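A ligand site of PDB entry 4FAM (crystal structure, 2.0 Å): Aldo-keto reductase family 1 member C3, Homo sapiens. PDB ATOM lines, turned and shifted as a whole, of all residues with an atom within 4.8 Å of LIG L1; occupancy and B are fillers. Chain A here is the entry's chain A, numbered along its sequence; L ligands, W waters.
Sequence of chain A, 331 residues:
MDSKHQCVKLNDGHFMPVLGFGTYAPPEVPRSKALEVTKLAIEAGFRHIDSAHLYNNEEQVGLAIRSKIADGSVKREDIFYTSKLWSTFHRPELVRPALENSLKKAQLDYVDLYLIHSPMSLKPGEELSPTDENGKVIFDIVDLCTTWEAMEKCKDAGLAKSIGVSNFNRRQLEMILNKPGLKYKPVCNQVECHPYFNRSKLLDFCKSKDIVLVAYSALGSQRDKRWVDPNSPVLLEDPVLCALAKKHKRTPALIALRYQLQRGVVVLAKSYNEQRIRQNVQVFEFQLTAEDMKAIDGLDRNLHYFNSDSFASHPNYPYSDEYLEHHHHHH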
ATOM      1  N   TYR A  24     -19.032  -3.388  26.609  1.00  0.00           N
ATOM      2  CA  TYR A  24     -18.365  -2.288  27.287  1.00  0.00           C
ATOM      3  C   TYR A  24     -18.520  -0.950  26.509  1.00  0.00           C
ATOM      4  O   TYR A  24     -18.193  -0.863  25.327  1.00  0.00           O
ATOM      5  CB  TYR A  24     -16.885  -2.519  27.538  1.00  0.00           C
ATOM      6  CG  TYR A  24     -16.245  -1.371  28.305  1.00  0.00           C
ATOM      7  CD1 TYR A  24     -16.493  -1.186  29.645  1.00  0.00           C
ATOM      8  CD2 TYR A  24     -15.502  -0.388  27.656  1.00  0.00           C
ATOM      9  CE1 TYR A  24     -15.974  -0.078  30.345  1.00  0.00           C
ATOM     10  CE2 TYR A  24     -14.947   0.724  28.356  1.00  0.00           C
ATOM     11  CZ  TYR A  24     -15.163   0.827  29.709  1.00  0.00           C
ATOM     12  OH  TYR A  24     -14.656   1.914  30.402  1.00  0.00           O
ATOM     13  N   LEU A  54     -16.854  -4.906  36.007  1.00  0.00           N
ATOM     14  CA  LEU A  54     -16.191  -3.659  35.643  1.00  0.00           C
ATOM     15  C   LEU A  54     -17.056  -2.715  34.807  1.00  0.00           C
ATOM     16  O   LEU A  54     -16.899  -1.457  34.909  1.00  0.00           O
ATOM     17  CB  LEU A  54     -14.892  -3.919  34.849  1.00  0.00           C
ATOM     18  CG  LEU A  54     -14.158  -2.656  34.323  1.00  0.00           C
ATOM     19  CD1 LEU A  54     -13.498  -1.919  35.512  1.00  0.00           C
ATOM     20  CD2 LEU A  54     -13.078  -3.134  33.333  1.00  0.00           C
ATOM     21  N   TYR A  55     -17.937  -3.284  33.965  1.00  0.00           N
ATOM     22  CA  TYR A  55     -18.580  -2.469  32.962  1.00  0.00           C
ATOM     23  C   TYR A  55     -19.707  -1.644  33.517  1.00  0.00           C
ATOM     24  O   TYR A  55     -20.183  -0.702  32.848  1.00  0.00           O
ATOM     25  CB  TYR A  55     -19.127  -3.336  31.809  1.00  0.00           C
ATOM     26  CG  TYR A  55     -18.073  -4.176  31.105  1.00  0.00           C
ATOM     27  CD1 TYR A  55     -16.729  -4.014  31.376  1.00  0.00           C
ATOM     28  CD2 TYR A  55     -18.436  -5.135  30.166  1.00  0.00           C
ATOM     29  CE1 TYR A  55     -15.779  -4.790  30.783  1.00  0.00           C
ATOM     30  CE2 TYR A  55     -17.498  -5.977  29.583  1.00  0.00           C
ATOM     31  CZ  TYR A  55     -16.181  -5.802  29.875  1.00  0.00           C
ATOM     32  OH  TYR A  55     -15.260  -6.607  29.299  1.00  0.00           O
ATOM     33  N   TRP A  86     -13.972  -9.053  38.915  1.00  0.00           N
ATOM     34  CA  TRP A  86     -13.089  -7.898  38.873  1.00  0.00           C
ATOM     35  C   TRP A  86     -11.898  -8.114  39.820  1.00  0.00           C
ATOM     36  O   TRP A  86     -11.978  -8.928  40.749  1.00  0.00           O
ATOM     37  CB  TRP A  86     -13.882  -6.634  39.154  1.00  0.00           C
ATOM     38  CG  TRP A  86     -13.022  -5.430  39.025  1.00  0.00           C
ATOM     39  CD1 TRP A  86     -12.697  -4.515  40.036  1.00  0.00           C
ATOM     40  CD2 TRP A  86     -12.158  -5.076  37.869  1.00  0.00           C
ATOM     41  NE1 TRP A  86     -11.761  -3.607  39.583  1.00  0.00           N
ATOM     42  CE2 TRP A  86     -11.360  -3.919  38.288  1.00  0.00           C
ATOM     43  CE3 TRP A  86     -11.926  -5.640  36.583  1.00  0.00           C
ATOM     44  CZ2 TRP A  86     -10.496  -3.243  37.430  1.00  0.00           C
ATOM     45  CZ3 TRP A  86     -10.984  -4.989  35.739  1.00  0.00           C
ATOM     46  CH2 TRP A  86     -10.291  -3.818  36.137  1.00  0.00           C
ATOM     47  N   HIS A 117     -11.244 -11.729  35.291  1.00  0.00           N
ATOM     48  CA  HIS A 117     -11.080 -10.663  34.302  1.00  0.00           C
ATOM     49  C   HIS A 117      -9.672 -10.395  33.908  1.00  0.00           C
ATOM     50  O   HIS A 117      -9.414 -10.127  32.755  1.00  0.00           O
ATOM     51  CB  HIS A 117     -11.698  -9.388  34.843  1.00  0.00           C
ATOM     52  CG  HIS A 117     -12.170  -8.426  33.788  1.00  0.00           C
ATOM     53  ND1 HIS A 117     -13.333  -7.698  33.957  1.00  0.00           N
ATOM     54  CD2 HIS A 117     -11.603  -8.024  32.581  1.00  0.00           C
ATOM     55  CE1 HIS A 117     -13.493  -6.878  32.879  1.00  0.00           C
ATOM     56  NE2 HIS A 117     -12.440  -7.071  32.025  1.00  0.00           N
ATOM     57  N   SER A 118      -8.752 -10.432  34.879  1.00  0.00           N
ATOM     58  CA  SER A 118      -7.351 -10.076  34.677  1.00  0.00           C
ATOM     59  C   SER A 118      -6.550 -10.740  35.775  1.00  0.00           C
ATOM     60  O   SER A 118      -7.034 -10.835  36.870  1.00  0.00           O
ATOM     61  CB  SER A 118      -7.153  -8.569  34.800  1.00  0.00           C
ATOM     62  OG  SER A 118      -5.801  -8.249  34.765  1.00  0.00           O
ATOM     63  N   MET A 120      -4.167  -9.288  37.206  1.00  0.00           N
ATOM     64  CA  MET A 120      -3.508  -8.180  37.929  1.00  0.00           C
ATOM     65  C   MET A 120      -4.323  -7.744  39.145  1.00  0.00           C
ATOM     66  O   MET A 120      -5.038  -6.760  39.165  1.00  0.00           O
ATOM     67  CB  MET A 120      -3.161  -7.003  36.962  1.00  0.00           C
ATOM     68  CG  MET A 120      -2.063  -7.388  35.984  1.00  0.00           C
ATOM     69  SD  MET A 120      -1.721  -6.148  34.706  1.00  0.00           S
ATOM     70  CE  MET A 120      -3.064  -6.473  33.564  1.00  0.00           C
ATOM     71  N   ASN A 167      -6.987 -12.305  29.922  1.00  0.00           N
ATOM     72  CA  ASN A 167      -5.701 -11.584  30.034  1.00  0.00           C
ATOM     73  C   ASN A 167      -4.617 -12.473  30.669  1.00  0.00           C
ATOM     74  O   ASN A 167      -3.684 -11.950  31.255  1.00  0.00           O
ATOM     75  CB  ASN A 167      -5.906 -10.298  30.787  1.00  0.00           C
ATOM     76  CG  ASN A 167      -6.742  -9.303  30.013  1.00  0.00           C
ATOM     77  OD1 ASN A 167      -6.373  -9.014  28.870  1.00  0.00           O
ATOM     78  ND2 ASN A 167      -7.911  -8.808  30.586  1.00  0.00           N
ATOM     79  N   TYR A 216     -10.856 -10.289  22.233  1.00  0.00           N
ATOM     80  CA  TYR A 216     -11.271  -8.887  22.397  1.00  0.00           C
ATOM     81  C   TYR A 216     -10.478  -7.889  21.626  1.00  0.00           C
ATOM     82  O   TYR A 216      -9.350  -8.116  21.124  1.00  0.00           O
ATOM     83  CB  TYR A 216     -11.416  -8.493  23.868  1.00  0.00           C
ATOM     84  CG  TYR A 216     -10.176  -8.264  24.672  1.00  0.00           C
ATOM     85  CD1 TYR A 216      -9.388  -7.142  24.458  1.00  0.00           C
ATOM     86  CD2 TYR A 216      -9.871  -9.052  25.774  1.00  0.00           C
ATOM     87  CE1 TYR A 216      -8.309  -6.834  25.279  1.00  0.00           C
ATOM     88  CE2 TYR A 216      -8.782  -8.738  26.576  1.00  0.00           C
ATOM     89  CZ  TYR A 216      -8.008  -7.618  26.323  1.00  0.00           C
ATOM     90  OH  TYR A 216      -6.948  -7.273  27.113  1.00  0.00           O
ATOM     91  N   TRP A 227      -6.428   4.341  27.714  1.00  0.00           N
ATOM     92  CA  TRP A 227      -5.724   3.041  27.580  1.00  0.00           C
ATOM     93  C   TRP A 227      -4.952   2.832  26.305  1.00  0.00           C
ATOM     94  O   TRP A 227      -4.212   1.891  26.248  1.00  0.00           O
ATOM     95  CB  TRP A 227      -6.774   1.919  27.572  1.00  0.00           C
ATOM     96  CG  TRP A 227      -7.583   1.888  28.837  1.00  0.00           C
ATOM     97  CD1 TRP A 227      -8.911   2.233  29.004  1.00  0.00           C
ATOM     98  CD2 TRP A 227      -7.096   1.555  30.125  1.00  0.00           C
ATOM     99  NE1 TRP A 227      -9.286   2.090  30.311  1.00  0.00           N
ATOM    100  CE2 TRP A 227      -8.226   1.673  31.036  1.00  0.00           C
ATOM    101  CE3 TRP A 227      -5.924   1.071  30.584  1.00  0.00           C
ATOM    102  CZ2 TRP A 227      -8.128   1.369  32.349  1.00  0.00           C
ATOM    103  CZ3 TRP A 227      -5.818   0.793  31.921  1.00  0.00           C
ATOM    104  CH2 TRP A 227      -6.885   0.962  32.781  1.00  0.00           C
ATOM    105  N   PHE A 306      -4.078  -1.841  24.305  1.00  0.00           N
ATOM    106  CA  PHE A 306      -4.040  -1.606  25.756  1.00  0.00           C
ATOM    107  C   PHE A 306      -2.626  -1.417  26.253  1.00  0.00           C
ATOM    108  O   PHE A 306      -1.730  -2.265  26.061  1.00  0.00           O
ATOM    109  CB  PHE A 306      -4.828  -2.664  26.564  1.00  0.00           C
ATOM    110  CG  PHE A 306      -6.341  -2.512  26.450  1.00  0.00           C
ATOM    111  CD1 PHE A 306      -7.038  -1.749  27.356  1.00  0.00           C
ATOM    112  CD2 PHE A 306      -7.076  -3.064  25.356  1.00  0.00           C
ATOM    113  CE1 PHE A 306      -8.412  -1.542  27.213  1.00  0.00           C
ATOM    114  CE2 PHE A 306      -8.427  -2.864  25.208  1.00  0.00           C
ATOM    115  CZ  PHE A 306      -9.117  -2.110  26.157  1.00  0.00           C
ATOM    116  N   ASN A 307      -2.429  -0.304  26.939  1.00  0.00           N
ATOM    117  CA  ASN A 307      -1.108   0.058  27.443  1.00  0.00           C
ATOM    118  C   ASN A 307      -1.318   0.823  28.718  1.00  0.00           C
ATOM    119  O   ASN A 307      -2.290   1.559  28.824  1.00  0.00           O
ATOM    120  CB  ASN A 307      -0.331   0.821  26.350  1.00  0.00           C
ATOM    121  CG  ASN A 307       1.142   0.490  26.328  1.00  0.00           C
ATOM    122  OD1 ASN A 307       1.562  -0.560  25.827  1.00  0.00           O
ATOM    123  ND2 ASN A 307       1.938   1.380  26.869  1.00  0.00           N
ATOM    124  N   SER A 308      -0.531   0.531  29.734  1.00  0.00           N
ATOM    125  CA  SER A 308      -0.589   1.179  31.055  1.00  0.00           C
ATOM    126  C   SER A 308       0.794   1.083  31.732  1.00  0.00           C
ATOM    127  O   SER A 308       1.237  -0.021  32.027  1.00  0.00           O
ATOM    128  CB  SER A 308      -1.626   0.514  31.954  1.00  0.00           C
ATOM    129  OG  SER A 308      -1.475   0.901  33.308  1.00  0.00           O
ATOM    130  N   PHE A 311       0.103  -0.712  35.094  1.00  0.00           N
ATOM    131  CA  PHE A 311      -0.020  -2.169  35.011  1.00  0.00           C
ATOM    132  C   PHE A 311       1.259  -2.817  34.572  1.00  0.00           C
ATOM    133  O   PHE A 311       1.510  -3.940  34.979  1.00  0.00           O
ATOM    134  CB  PHE A 311      -1.220  -2.654  34.176  1.00  0.00           C
ATOM    135  CG  PHE A 311      -2.553  -2.296  34.761  1.00  0.00           C
ATOM    136  CD1 PHE A 311      -2.725  -2.208  36.117  1.00  0.00           C
ATOM    137  CD2 PHE A 311      -3.641  -2.082  33.964  1.00  0.00           C
ATOM    138  CE1 PHE A 311      -3.950  -1.848  36.660  1.00  0.00           C
ATOM    139  CE2 PHE A 311      -4.866  -1.709  34.496  1.00  0.00           C
ATOM    140  CZ  PHE A 311      -5.005  -1.565  35.850  1.00  0.00           C
ATOM    141  N   TYR A 317       1.578  -8.761  35.330  1.00  0.00           N
ATOM    142  CA  TYR A 317       1.398  -8.158  34.022  1.00  0.00           C
ATOM    143  C   TYR A 317       1.588  -9.198  32.931  1.00  0.00           C
ATOM    144  O   TYR A 317       2.603  -9.844  32.907  1.00  0.00           O
ATOM    145  CB  TYR A 317       2.412  -7.058  33.803  1.00  0.00           C
ATOM    146  CG  TYR A 317       2.317  -6.306  32.481  1.00  0.00           C
ATOM    147  CD1 TYR A 317       1.154  -5.594  32.113  1.00  0.00           C
ATOM    148  CD2 TYR A 317       3.414  -6.248  31.597  1.00  0.00           C
ATOM    149  CE1 TYR A 317       1.102  -4.867  30.917  1.00  0.00           C
ATOM    150  CE2 TYR A 317       3.348  -5.522  30.399  1.00  0.00           C
ATOM    151  CZ  TYR A 317       2.196  -4.825  30.095  1.00  0.00           C
ATOM    152  OH  TYR A 317       2.122  -4.077  28.931  1.00  0.00           O
ATOM    153  N   TYR A 319       2.107  -9.126  29.631  1.00  0.00           N
ATOM    154  CA  TYR A 319       2.878  -8.858  28.392  1.00  0.00           C
ATOM    155  C   TYR A 319       4.406  -8.772  28.519  1.00  0.00           C
ATOM    156  O   TYR A 319       5.085  -8.683  27.506  1.00  0.00           O
ATOM    157  CB  TYR A 319       2.333  -7.617  27.694  1.00  0.00           C
ATOM    158  CG  TYR A 319       0.901  -7.754  27.230  1.00  0.00           C
ATOM    159  CD1 TYR A 319       0.474  -8.898  26.557  1.00  0.00           C
ATOM    160  CD2 TYR A 319      -0.010  -6.700  27.377  1.00  0.00           C
ATOM    161  CE1 TYR A 319      -0.855  -9.016  26.108  1.00  0.00           C
ATOM    162  CE2 TYR A 319      -1.318  -6.782  26.918  1.00  0.00           C
ATOM    163  CZ  TYR A 319      -1.707  -7.941  26.241  1.00  0.00           C
ATOM    164  OH  TYR A 319      -2.959  -8.087  25.819  1.00  0.00           O
HETATM  165  O1  LIG L   1     -13.642  -4.071  28.288  1.00  0.00           O
HETATM  166  C1  LIG L   1     -12.758  -4.419  29.150  1.00  0.00           C
HETATM  167  O2  LIG L   1     -13.020  -5.491  29.811  1.00  0.00           O
HETATM  168  C2  LIG L   1     -11.765  -3.513  29.639  1.00  0.00           C
HETATM  169  C3  LIG L   1     -10.780  -3.927  30.529  1.00  0.00           C
HETATM  170  C4  LIG L   1     -11.849  -2.128  29.350  1.00  0.00           C
HETATM  171  C5  LIG L   1     -10.950  -1.207  29.946  1.00  0.00           C
HETATM  172  C6  LIG L   1      -9.966  -1.682  30.828  1.00  0.00           C
HETATM  173  C7  LIG L   1      -9.875  -3.055  31.114  1.00  0.00           C
HETATM  174  S1  LIG L   1      -8.772  -3.608  32.209  1.00  0.00           S
HETATM  175  O3  LIG L   1      -9.171  -4.940  32.632  1.00  0.00           O
HETATM  176  O4  LIG L   1      -8.424  -2.527  33.104  1.00  0.00           O
HETATM  177  N1  LIG L   1      -7.337  -3.908  31.524  1.00  0.00           N
HETATM  178  C8  LIG L   1      -7.387  -4.846  30.360  1.00  0.00           C
HETATM  179  C9  LIG L   1      -6.040  -5.518  30.266  1.00  0.00           C
HETATM  180  C10 LIG L   1      -4.976  -4.561  30.151  1.00  0.00           C
HETATM  181  C11 LIG L   1      -3.717  -4.988  29.685  1.00  0.00           C
HETATM  182  C12 LIG L   1      -2.675  -4.096  29.527  1.00  0.00           C
HETATM  183  C13 LIG L   1      -2.886  -2.775  29.867  1.00  0.00           C
HETATM  184  C14 LIG L   1      -4.110  -2.357  30.344  1.00  0.00           C
HETATM  185  C15 LIG L   1      -5.182  -3.254  30.510  1.00  0.00           C
HETATM  186  C16 LIG L   1      -6.469  -2.781  31.029  1.00  0.00           C
HETATM  187  P1  LG2 L   2     -14.020  -3.704  19.427  1.00  0.00           P
HETATM  188  O1  LG2 L   2     -14.925  -4.926  19.262  1.00  0.00           O
HETATM  189  O2  LG2 L   2     -12.622  -3.882  19.159  1.00  0.00           O
HETATM  190  O3  LG2 L   2     -14.645  -2.479  18.622  1.00  0.00           O
HETATM  191  C1  LG2 L   2     -13.864  -1.297  18.460  1.00  0.00           C
HETATM  192  C2  LG2 L   2     -14.759  -0.158  17.788  1.00  0.00           C
HETATM  193  O4  LG2 L   2     -15.169  -0.843  16.551  1.00  0.00           O
HETATM  194  C3  LG2 L   2     -16.063  -0.048  18.513  1.00  0.00           C
HETATM  195  O5  LG2 L   2     -16.054   1.059  19.469  1.00  0.00           O
HETATM  196  C4  LG2 L   2     -17.138   0.170  17.445  1.00  0.00           C
HETATM  197  O6  LG2 L   2     -17.583   1.559  17.431  1.00  0.00           O
HETATM  198  C5  LG2 L   2     -16.427  -0.159  16.122  1.00  0.00           C
HETATM  199  N1  LG2 L   2     -17.159  -1.006  15.218  1.00  0.00           N
HETATM  200  C6  LG2 L   2     -17.896  -2.105  15.535  1.00  0.00           C
HETATM  201  N2  LG2 L   2     -18.351  -2.726  14.439  1.00  0.00           N
HETATM  202  C7  LG2 L   2     -17.910  -1.992  13.423  1.00  0.00           C
HETATM  203  C8  LG2 L   2     -18.091  -2.103  12.070  1.00  0.00           C
HETATM  204  N3  LG2 L   2     -18.885  -3.010  11.561  1.00  0.00           N
HETATM  205  N4  LG2 L   2     -17.526  -1.147  11.184  1.00  0.00           N
HETATM  206  C9  LG2 L   2     -16.704  -0.039  11.653  1.00  0.00           C
HETATM  207  N5  LG2 L   2     -16.532  -0.036  13.058  1.00  0.00           N
HETATM  208  C10 LG2 L   2     -17.114  -0.952  13.900  1.00  0.00           C
HETATM  209  O7  LG2 L   2     -14.218  -3.112  20.866  1.00  0.00           O
HETATM  210  P2  LG2 L   2     -13.644  -3.566  22.359  1.00  0.00           P
HETATM  211  O8  LG2 L   2     -14.529  -2.981  23.350  1.00  0.00           O
HETATM  212  O9  LG2 L   2     -12.245  -3.205  22.521  1.00  0.00           O
HETATM  213  O10 LG2 L   2     -13.733  -5.196  22.326  1.00  0.00           O
HETATM  214  C11 LG2 L   2     -15.026  -5.713  22.437  1.00  0.00           C
HETATM  215  C12 LG2 L   2     -15.575  -6.339  23.722  1.00  0.00           C
HETATM  216  O11 LG2 L   2     -14.495  -7.206  24.177  1.00  0.00           O
HETATM  217  C13 LG2 L   2     -15.711  -5.261  24.854  1.00  0.00           C
HETATM  218  O12 LG2 L   2     -16.932  -4.530  24.593  1.00  0.00           O
HETATM  219  C14 LG2 L   2     -15.781  -6.249  25.998  1.00  0.00           C
HETATM  220  O13 LG2 L   2     -16.989  -7.018  26.035  1.00  0.00           O
HETATM  221  C15 LG2 L   2     -14.585  -7.207  25.598  1.00  0.00           C
HETATM  222  N6  LG2 L   2     -13.314  -6.779  26.148  1.00  0.00           N
HETATM  223  C16 LG2 L   2     -12.713  -7.479  27.211  1.00  0.00           C
HETATM  224  C17 LG2 L   2     -11.513  -7.047  27.752  1.00  0.00           C
HETATM  225  C18 LG2 L   2     -10.873  -7.793  28.854  1.00  0.00           C
HETATM  226  O14 LG2 L   2      -9.944  -7.287  29.465  1.00  0.00           O
HETATM  227  N7  LG2 L   2     -11.287  -9.055  28.937  1.00  0.00           N
HETATM  228  C19 LG2 L   2     -10.864  -5.980  27.182  1.00  0.00           C
HETATM  229  C20 LG2 L   2     -11.496  -5.276  26.130  1.00  0.00           C
HETATM  230  C21 LG2 L   2     -12.634  -5.716  25.568  1.00  0.00           C
HETATM  231  P3  LG2 L   2     -19.196   1.831  17.495  1.00  0.00           P
HETATM  232  O15 LG2 L   2     -19.824   1.476  18.779  1.00  0.00           O
HETATM  233  O16 LG2 L   2     -19.330   3.240  16.997  1.00  0.00           O
HETATM  234  O17 LG2 L   2     -19.823   0.977  16.377  1.00  0.00           O
HETATM  235  O   HOH W   1     -13.408  -2.302  25.962  1.00  0.00           O
HETATM  236  O   HOH W   2     -10.025  -0.417  34.582  1.00  0.00           O
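Merely in contact with LIG L1: Trp 86, Phe 311, Tyr 24, Leu 54, Trp 227, Tyr 216, Phe 306, Asn 167, Asn 307 and Tyr 319. Hydrophobic or aromatic side chains within 4 Å of LIG L1: Tyr 24, Leu 54, Tyr 55, Trp 86, His 117, Trp 227, Phe 306, Phe 311 and Tyr 319. Of the 16 residues printed, 12 come within 4 Å of LIG L1. Along chain A the residues within 4 Å of LIG L1 span positions 24 to 319.
Water W1 lies within hydrogen-bond range of an oxygen (O8) of LG2 L2 (2.9 Å) and an oxygen (O1) of LIG L1 (2.9 Å).
The backbone carbonyl oxygen (O) of Trp 227 sits at hydrogen-bond distance from the backbone NH (N) of Asn 307 (2.9 Å). OG of Ser 308 lies within hydrogen-bond range of N of Phe 311. OH of Tyr 216 sits at hydrogen-bond distance from OD1 of Asn 167, at 2.5 Å. The backbone carbonyl oxygen (O) of His 117 lies within hydrogen-bond range of the side-chain amide nitrogen (ND2) of Asn 167 (3.0 Å).
A ring nitrogen (NE2) of His 117 sits at hydrogen-bond distance from an oxygen (O2) of LIG L1, at 2.8 Å. The side-chain amide nitrogen of Asn 167 sits at hydrogen-bond distance from an oxygen (O14) of LG2 L2 (2.8 Å). N of Tyr 24 lies within hydrogen-bond range of O12 of LG2 L2. An oxygen (O2) of LIG L1 sits at hydrogen-bond distance from the side-chain hydroxyl (OH) of Tyr 55.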
